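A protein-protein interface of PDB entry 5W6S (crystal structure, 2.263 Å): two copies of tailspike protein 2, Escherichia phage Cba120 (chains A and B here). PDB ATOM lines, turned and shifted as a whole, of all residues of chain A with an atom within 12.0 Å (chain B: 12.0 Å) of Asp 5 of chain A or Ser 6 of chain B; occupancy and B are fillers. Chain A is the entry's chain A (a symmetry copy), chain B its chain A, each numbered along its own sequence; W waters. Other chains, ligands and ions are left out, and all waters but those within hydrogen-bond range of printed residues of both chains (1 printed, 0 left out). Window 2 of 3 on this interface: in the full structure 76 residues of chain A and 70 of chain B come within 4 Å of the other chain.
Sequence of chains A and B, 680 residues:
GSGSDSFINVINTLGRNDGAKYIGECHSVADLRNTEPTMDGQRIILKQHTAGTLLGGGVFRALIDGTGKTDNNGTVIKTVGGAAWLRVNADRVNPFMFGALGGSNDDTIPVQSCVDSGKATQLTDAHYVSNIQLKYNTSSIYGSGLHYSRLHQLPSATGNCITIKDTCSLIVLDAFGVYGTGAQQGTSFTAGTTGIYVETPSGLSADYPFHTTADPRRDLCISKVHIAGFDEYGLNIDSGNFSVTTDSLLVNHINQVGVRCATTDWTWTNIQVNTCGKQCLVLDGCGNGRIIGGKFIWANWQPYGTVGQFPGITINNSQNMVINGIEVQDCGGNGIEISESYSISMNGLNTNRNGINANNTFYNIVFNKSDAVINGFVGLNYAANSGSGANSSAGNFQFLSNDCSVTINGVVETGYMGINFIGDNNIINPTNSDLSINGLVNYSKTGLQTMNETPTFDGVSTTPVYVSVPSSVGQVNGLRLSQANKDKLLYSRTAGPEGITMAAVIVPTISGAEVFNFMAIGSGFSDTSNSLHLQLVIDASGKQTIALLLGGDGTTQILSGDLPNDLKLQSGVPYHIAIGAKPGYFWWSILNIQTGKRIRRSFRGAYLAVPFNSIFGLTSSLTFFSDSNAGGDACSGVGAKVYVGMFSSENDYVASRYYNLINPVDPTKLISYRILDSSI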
ATOM      1  N   ASP A   5      17.639  30.994  33.567  1.00  0.00           N
ATOM      2  CA  ASP A   5      16.965  29.711  33.402  1.00  0.00           C
ATOM      3  C   ASP A   5      17.981  28.578  33.290  1.00  0.00           C
ATOM      4  O   ASP A   5      18.757  28.521  32.337  1.00  0.00           O
ATOM      5  CB  ASP A   5      16.060  29.736  32.168  1.00  0.00           C
ATOM      6  CG  ASP A   5      14.859  28.819  32.307  1.00  0.00           C
ATOM      7  OD1 ASP A   5      14.986  27.760  32.956  1.00  0.00           O
ATOM      8  OD2 ASP A   5      13.786  29.166  31.769  1.00  0.00           O
ATOM      9  N   SER A   6      17.970  27.671  34.270  1.00  0.00           N
ATOM     10  CA  SER A   6      18.928  26.571  34.282  1.00  0.00           C
ATOM     11  C   SER A   6      18.769  25.636  33.088  1.00  0.00           C
ATOM     12  O   SER A   6      19.588  24.723  32.925  1.00  0.00           O
ATOM     13  CB  SER A   6      18.803  25.775  35.585  1.00  0.00           C
ATOM     14  OG  SER A   6      17.535  25.150  35.687  1.00  0.00           O
ATOM     15  N   PHE A   7      17.740  25.831  32.261  1.00  0.00           N
ATOM     16  CA  PHE A   7      17.623  25.059  31.028  1.00  0.00           C
ATOM     17  C   PHE A   7      18.709  25.455  30.035  1.00  0.00           C
ATOM     18  O   PHE A   7      19.417  24.596  29.494  1.00  0.00           O
ATOM     19  CB  PHE A   7      16.232  25.255  30.424  1.00  0.00           C
ATOM     20  CG  PHE A   7      16.087  24.706  29.032  1.00  0.00           C
ATOM     21  CD1 PHE A   7      15.825  23.361  28.828  1.00  0.00           C
ATOM     22  CD2 PHE A   7      16.207  25.534  27.930  1.00  0.00           C
ATOM     23  CE1 PHE A   7      15.691  22.855  27.549  1.00  0.00           C
ATOM     24  CE2 PHE A   7      16.075  25.032  26.650  1.00  0.00           C
ATOM     25  CZ  PHE A   7      15.816  23.692  26.461  1.00  0.00           C
ATOM     26  N   ILE A   8      18.852  26.760  29.787  1.00  0.00           N
ATOM     27  CA  ILE A   8      19.930  27.254  28.935  1.00  0.00           C
ATOM     28  C   ILE A   8      21.284  26.817  29.480  1.00  0.00           C
ATOM     29  O   ILE A   8      22.190  26.453  28.720  1.00  0.00           O
ATOM     30  CB  ILE A   8      19.836  28.786  28.806  1.00  0.00           C
ATOM     31  CG1 ILE A   8      18.625  29.172  27.955  1.00  0.00           C
ATOM     32  CG2 ILE A   8      21.120  29.361  28.231  1.00  0.00           C
ATOM     33  CD1 ILE A   8      18.392  30.669  27.867  1.00  0.00           C
ATOM     34  N   ASN A   9      21.445  26.843  30.803  1.00  0.00           N
ATOM     35  CA  ASN A   9      22.699  26.395  31.398  1.00  0.00           C
ATOM     36  C   ASN A   9      23.017  24.959  31.006  1.00  0.00           C
ATOM     37  O   ASN A   9      24.170  24.634  30.694  1.00  0.00           O
ATOM     38  CB  ASN A   9      22.638  26.532  32.917  1.00  0.00           C
ATOM     39  CG  ASN A   9      22.851  27.949  33.375  1.00  0.00           C
ATOM     40  OD1 ASN A   9      22.982  28.858  32.555  1.00  0.00           O
ATOM     41  ND2 ASN A   9      22.884  28.154  34.688  1.00  0.00           N
ATOM     42  N   VAL A  10      22.014  24.082  31.023  1.00  0.00           N
ATOM     43  CA  VAL A  10      22.262  22.680  30.705  1.00  0.00           C
ATOM     44  C   VAL A  10      22.599  22.517  29.229  1.00  0.00           C
ATOM     45  O   VAL A  10      23.523  21.777  28.870  1.00  0.00           O
ATOM     46  CB  VAL A  10      21.058  21.814  31.111  1.00  0.00           C
ATOM     47  CG1 VAL A  10      21.241  20.395  30.607  1.00  0.00           C
ATOM     48  CG2 VAL A  10      20.896  21.823  32.621  1.00  0.00           C
ATOM     49  N   ILE A  11      21.865  23.202  28.349  1.00  0.00           N
ATOM     50  CA  ILE A  11      22.150  23.095  26.922  1.00  0.00           C
ATOM     51  C   ILE A  11      23.545  23.628  26.615  1.00  0.00           C
ATOM     52  O   ILE A  11      24.312  23.009  25.868  1.00  0.00           O
ATOM     53  CB  ILE A  11      21.065  23.814  26.097  1.00  0.00           C
ATOM     54  CG1 ILE A  11      19.955  22.835  25.706  1.00  0.00           C
ATOM     55  CG2 ILE A  11      21.668  24.436  24.848  1.00  0.00           C
ATOM     56  CD1 ILE A  11      19.263  22.179  26.878  1.00  0.00           C
ATOM     57  N   ASN A  12      23.905  24.775  27.196  1.00  0.00           N
ATOM     58  CA  ASN A  12      25.232  25.324  26.940  1.00  0.00           C
ATOM     59  C   ASN A  12      26.324  24.446  27.545  1.00  0.00           C
ATOM     60  O   ASN A  12      27.402  24.296  26.955  1.00  0.00           O
ATOM     61  CB  ASN A  12      25.317  26.757  27.461  1.00  0.00           C
ATOM     62  CG  ASN A  12      24.480  27.722  26.638  1.00  0.00           C
ATOM     63  OD1 ASN A  12      24.030  27.387  25.544  1.00  0.00           O
ATOM     64  ND2 ASN A  12      24.267  28.924  27.159  1.00  0.00           N
ATOM     65  N   THR A  13      26.064  23.841  28.706  1.00  0.00           N
ATOM     66  CA  THR A  13      27.056  22.944  29.294  1.00  0.00           C
ATOM     67  C   THR A  13      27.224  21.681  28.460  1.00  0.00           C
ATOM     68  O   THR A  13      28.352  21.240  28.211  1.00  0.00           O
ATOM     69  CB  THR A  13      26.666  22.579  30.726  1.00  0.00           C
ATOM     70  OG1 THR A  13      26.761  23.737  31.557  1.00  0.00           O
ATOM     71  CG2 THR A  13      27.592  21.492  31.267  1.00  0.00           C
ATOM     72  N   LEU A  14      26.117  21.074  28.032  1.00  0.00           N
ATOM     73  CA  LEU A  14      26.219  19.882  27.200  1.00  0.00           C
ATOM     74  C   LEU A  14      26.822  20.203  25.839  1.00  0.00           C
ATOM     75  O   LEU A  14      27.481  19.346  25.237  1.00  0.00           O
ATOM     76  CB  LEU A  14      24.842  19.245  27.039  1.00  0.00           C
ATOM     77  CG  LEU A  14      24.280  18.634  28.318  1.00  0.00           C
ATOM     78  CD1 LEU A  14      22.867  18.108  28.090  1.00  0.00           C
ATOM     79  CD2 LEU A  14      25.201  17.526  28.803  1.00  0.00           C
ATOM     80  N   ASP B   5       8.784  22.604  35.550  1.00  0.00           N
ATOM     81  CA  ASP B   5      10.133  22.243  35.973  1.00  0.00           C
ATOM     82  C   ASP B   5      11.054  22.085  34.766  1.00  0.00           C
ATOM     83  O   ASP B   5      10.859  21.196  33.939  1.00  0.00           O
ATOM     84  CB  ASP B   5      10.109  20.953  36.796  1.00  0.00           C
ATOM     85  CG  ASP B   5      11.226  20.892  37.819  1.00  0.00           C
ATOM     86  OD1 ASP B   5      12.322  21.427  37.543  1.00  0.00           O
ATOM     87  OD2 ASP B   5      11.003  20.315  38.904  1.00  0.00           O
ATOM     88  N   SER B   6      12.064  22.953  34.672  1.00  0.00           N
ATOM     89  CA  SER B   6      12.978  22.917  33.535  1.00  0.00           C
ATOM     90  C   SER B   6      13.770  21.616  33.456  1.00  0.00           C
ATOM     91  O   SER B   6      14.503  21.416  32.479  1.00  0.00           O
ATOM     92  CB  SER B   6      13.940  24.108  33.592  1.00  0.00           C
ATOM     93  OG  SER B   6      14.778  24.039  34.732  1.00  0.00           O
ATOM     94  N   PHE B   7      13.652  20.738  34.454  1.00  0.00           N
ATOM     95  CA  PHE B   7      14.273  19.421  34.360  1.00  0.00           C
ATOM     96  C   PHE B   7      13.578  18.567  33.306  1.00  0.00           C
ATOM     97  O   PHE B   7      14.230  17.990  32.427  1.00  0.00           O
ATOM     98  CB  PHE B   7      14.243  18.735  35.727  1.00  0.00           C
ATOM     99  CG  PHE B   7      14.631  17.283  35.690  1.00  0.00           C
ATOM    100  CD1 PHE B   7      15.965  16.909  35.696  1.00  0.00           C
ATOM    101  CD2 PHE B   7      13.664  16.294  35.656  1.00  0.00           C
ATOM    102  CE1 PHE B   7      16.324  15.575  35.664  1.00  0.00           C
ATOM    103  CE2 PHE B   7      14.018  14.959  35.623  1.00  0.00           C
ATOM    104  CZ  PHE B   7      15.349  14.601  35.627  1.00  0.00           C
ATOM    105  N   ILE B   8      12.247  18.479  33.384  1.00  0.00           N
ATOM    106  CA  ILE B   8      11.474  17.776  32.365  1.00  0.00           C
ATOM    107  C   ILE B   8      11.739  18.373  30.988  1.00  0.00           C
ATOM    108  O   ILE B   8      11.846  17.650  29.989  1.00  0.00           O
ATOM    109  CB  ILE B   8       9.977  17.813  32.723  1.00  0.00           C
ATOM    110  CG1 ILE B   8       9.699  16.917  33.931  1.00  0.00           C
ATOM    111  CG2 ILE B   8       9.124  17.409  31.531  1.00  0.00           C
ATOM    112  CD1 ILE B   8       8.265  16.981  34.423  1.00  0.00           C
ATOM    113  N   ASN B   9      11.851  19.699  30.911  1.00  0.00           N
ATOM    114  CA  ASN B   9      12.149  20.336  29.634  1.00  0.00           C
ATOM    115  C   ASN B   9      13.450  19.812  29.042  1.00  0.00           C
ATOM    116  O   ASN B   9      13.533  19.557  27.834  1.00  0.00           O
ATOM    117  CB  ASN B   9      12.215  21.852  29.806  1.00  0.00           C
ATOM    118  CG  ASN B   9      10.850  22.481  29.876  1.00  0.00           C
ATOM    119  OD1 ASN B   9       9.838  21.782  29.862  1.00  0.00           O
ATOM    120  ND2 ASN B   9      10.808  23.808  29.955  1.00  0.00           N
ATOM    121  N   VAL B  10      14.480  19.651  29.873  1.00  0.00           N
ATOM    122  CA  VAL B  10      15.769  19.198  29.361  1.00  0.00           C
ATOM    123  C   VAL B  10      15.687  17.744  28.914  1.00  0.00           C
ATOM    124  O   VAL B  10      16.208  17.378  27.855  1.00  0.00           O
ATOM    125  CB  VAL B  10      16.871  19.409  30.412  1.00  0.00           C
ATOM    126  CG1 VAL B  10      18.164  18.764  29.950  1.00  0.00           C
ATOM    127  CG2 VAL B  10      17.077  20.892  30.660  1.00  0.00           C
ATOM    128  N   ILE B  11      15.033  16.892  29.707  1.00  0.00           N
ATOM    129  CA  ILE B  11      14.911  15.489  29.325  1.00  0.00           C
ATOM    130  C   ILE B  11      14.115  15.354  28.033  1.00  0.00           C
ATOM    131  O   ILE B  11      14.497  14.605  27.126  1.00  0.00           O
ATOM    132  CB  ILE B  11      14.290  14.667  30.472  1.00  0.00           C
ATOM    133  CG1 ILE B  11      15.387  14.083  31.365  1.00  0.00           C
ATOM    134  CG2 ILE B  11      13.424  13.547  29.918  1.00  0.00           C
ATOM    135  CD1 ILE B  11      16.293  15.115  31.996  1.00  0.00           C
ATOM    136  N   ASN B  12      13.004  16.087  27.917  1.00  0.00           N
ATOM    137  CA  ASN B  12      12.211  16.000  26.697  1.00  0.00           C
ATOM    138  C   ASN B  12      12.958  16.586  25.502  1.00  0.00           C
ATOM    139  O   ASN B  12      12.847  16.070  24.383  1.00  0.00           O
ATOM    140  CB  ASN B  12      10.860  16.684  26.899  1.00  0.00           C
ATOM    141  CG  ASN B  12       9.956  15.911  27.846  1.00  0.00           C
ATOM    142  OD1 ASN B  12      10.225  14.754  28.165  1.00  0.00           O
ATOM    143  ND2 ASN B  12       8.883  16.545  28.299  1.00  0.00           N
ATOM    144  N   THR B  13      13.738  17.647  25.717  1.00  0.00           N
ATOM    145  CA  THR B  13      14.519  18.208  24.617  1.00  0.00           C
ATOM    146  C   THR B  13      15.622  17.252  24.179  1.00  0.00           C
ATOM    147  O   THR B  13      15.830  17.045  22.977  1.00  0.00           O
ATOM    148  CB  THR B  13      15.121  19.554  25.017  1.00  0.00           C
ATOM    149  OG1 THR B  13      14.076  20.515  25.179  1.00  0.00           O
ATOM    150  CG2 THR B  13      16.094  20.041  23.945  1.00  0.00           C
ATOM    151  N   LEU B  14      16.350  16.674  25.133  1.00  0.00           N
ATOM    152  CA  LEU B  14      17.394  15.723  24.772  1.00  0.00           C
ATOM    153  C   LEU B  14      16.809  14.458  24.159  1.00  0.00           C
ATOM    154  O   LEU B  14      17.459  13.817  23.323  1.00  0.00           O
ATOM    155  CB  LEU B  14      18.231  15.384  26.002  1.00  0.00           C
ATOM    156  CG  LEU B  14      19.083  16.538  26.519  1.00  0.00           C
ATOM    157  CD1 LEU B  14      19.810  16.141  27.800  1.00  0.00           C
ATOM    158  CD2 LEU B  14      20.070  16.965  25.445  1.00  0.00           C
ATOM    159  N   GLY B  15      15.592  14.088  24.553  1.00  0.00           N
ATOM    160  CA  GLY B  15      14.954  12.879  24.092  1.00  0.00           C
ATOM    161  C   GLY B  15      14.328  12.947  22.723  1.00  0.00           C
ATOM    162  O   GLY B  15      13.792  11.940  22.256  1.00  0.00           O
ATOM    163  N   TYR B  22      22.604  17.973  20.657  1.00  0.00           N
ATOM    164  CA  TYR B  22      22.866  18.768  21.849  1.00  0.00           C
ATOM    165  C   TYR B  22      24.148  18.373  22.567  1.00  0.00           C
ATOM    166  O   TYR B  22      24.580  19.095  23.468  1.00  0.00           O
ATOM    167  CB  TYR B  22      21.683  18.666  22.805  1.00  0.00           C
ATOM    168  CG  TYR B  22      20.430  19.261  22.220  1.00  0.00           C
ATOM    169  CD1 TYR B  22      20.344  20.625  21.978  1.00  0.00           C
ATOM    170  CD2 TYR B  22      19.339  18.465  21.898  1.00  0.00           C
ATOM    171  CE1 TYR B  22      19.207  21.184  21.437  1.00  0.00           C
ATOM    172  CE2 TYR B  22      18.192  19.019  21.353  1.00  0.00           C
ATOM    173  CZ  TYR B  22      18.134  20.379  21.124  1.00  0.00           C
ATOM    174  OH  TYR B  22      17.003  20.945  20.583  1.00  0.00           O
HETATM  175  O   HOH W   1      23.484  21.519  23.667  1.00  0.00           O
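The side-chain hydroxyl (OG) of Ser 6 of chain B lies within hydrogen-bond range of the side-chain hydroxyl (OG) of Ser 6 of chain A, 3.1 Å away.
The backbone carbonyl oxygen of Leu 14 of chain A lies close to the backbone carbonyl oxygen of Tyr 22 of chain B, at 3.4 Å.
The backbone carbonyl oxygen of Asn 9 of chain B sits at hydrogen-bond distance from the side-chain hydroxyl of Thr 13 of chain B, at 2.9 Å.
N of Phe 7 of chain A sits close to OD1 of Asp 5 of chain A (3.4 Å).
Among the printed residues, merely in contact across the chains: Asp 5 of chain A with Ser 6 of chain B (3.9 Å), Phe 7 of chain A with Asn 9 of chain B (3.95 Å), Phe 7 of chain A with Val 10 of chain B (3.3 Å), Phe 7 of chain A with Thr 13 of chain B (3.7 Å), Val 10 of chain A with Val 10 of chain B (3.5 Å) and Leu 14 of chain A with Leu 14 of chain B (3.6 Å).
Of chain B, only Ser 6 (3.9 Å) comes within 4 Å of Asp 5 of chain A.
Printed residues of chain A within 4 Å of Ser 6 of chain B: Asp 5 and Ser 6.
Phe 7 of chain A touches three residues of chain B.
No residue of chain B comes within 4 Å of Ile 8 of chain A.
No residue of chain B comes within 4 Å of Asn 9 of chain A.
No residue of chain A comes within 4 Å of Asp 5 of chain B.
No residue of chain A comes within 4 Å of Phe 7 of chain B.
Ile 8 of chain B touches none of the printed residues of chain A.
Of chain A, only Phe 7 comes within 4 Å of Asn 9 of chain B.
Val 10 of chain B touches just these residues of chain A: Phe 7 and Val 10.
Printed residues of chain A within 4 Å of Thr 13 of chain B: Phe 7.
Printed residues of chain A within 4 Å of Leu 14 of chain B: Leu 14.
Of the printed residues of chain B, Val 10 of chain A touches Val 10 (3.5 Å).
Of the printed residues of chain B, Leu 14 of chain A touches Leu 14 and Tyr 22.
Printed residues of chain A within 4 Å of Tyr 22 of chain B: Leu 14 (3.4 Å).
Thr 13 of chain A touches none of the printed residues of chain B.
Asn 12 of chain B touches none of the printed residues of chain A.
The nearest residue of chain A that does not touch Ser 6 of chain B is Phe 7 of chain A (4.1 Å).
Printed residues of chain B that touch a printed residue of chain A: Ser 6, Asn 9, Val 10, Thr 13, Leu 14 and Tyr 22.
Hydrophobic or aromatic side chains of chain A that line the printed part of chain B: Phe 7, Val 10 and Leu 14.
Ser 6 of chain B touches its own counterpart, Ser 6 of chain A.
Phe 7 of chain A touches Thr 13 of chain B, but with the chains exchanged Thr 13 of chain A does not touch Phe 7 of chain B (13.1 Å).
Val 10 of chain A touches its own counterpart, Val 10 of chain B.
Leu 14 of chain B touches its own counterpart, Leu 14 of chain A.
10 positions are printed for both chains.
Of the 8 pairs that touch across the chains among the printed residues, 3 have their exchanged pair printed and touching as well.
Water W1 lies within hydrogen-bond range of the backbone carbonyl oxygen of Tyr 22 of chain B and the backbone carbonyl oxygen of Ile 11 of chain A.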
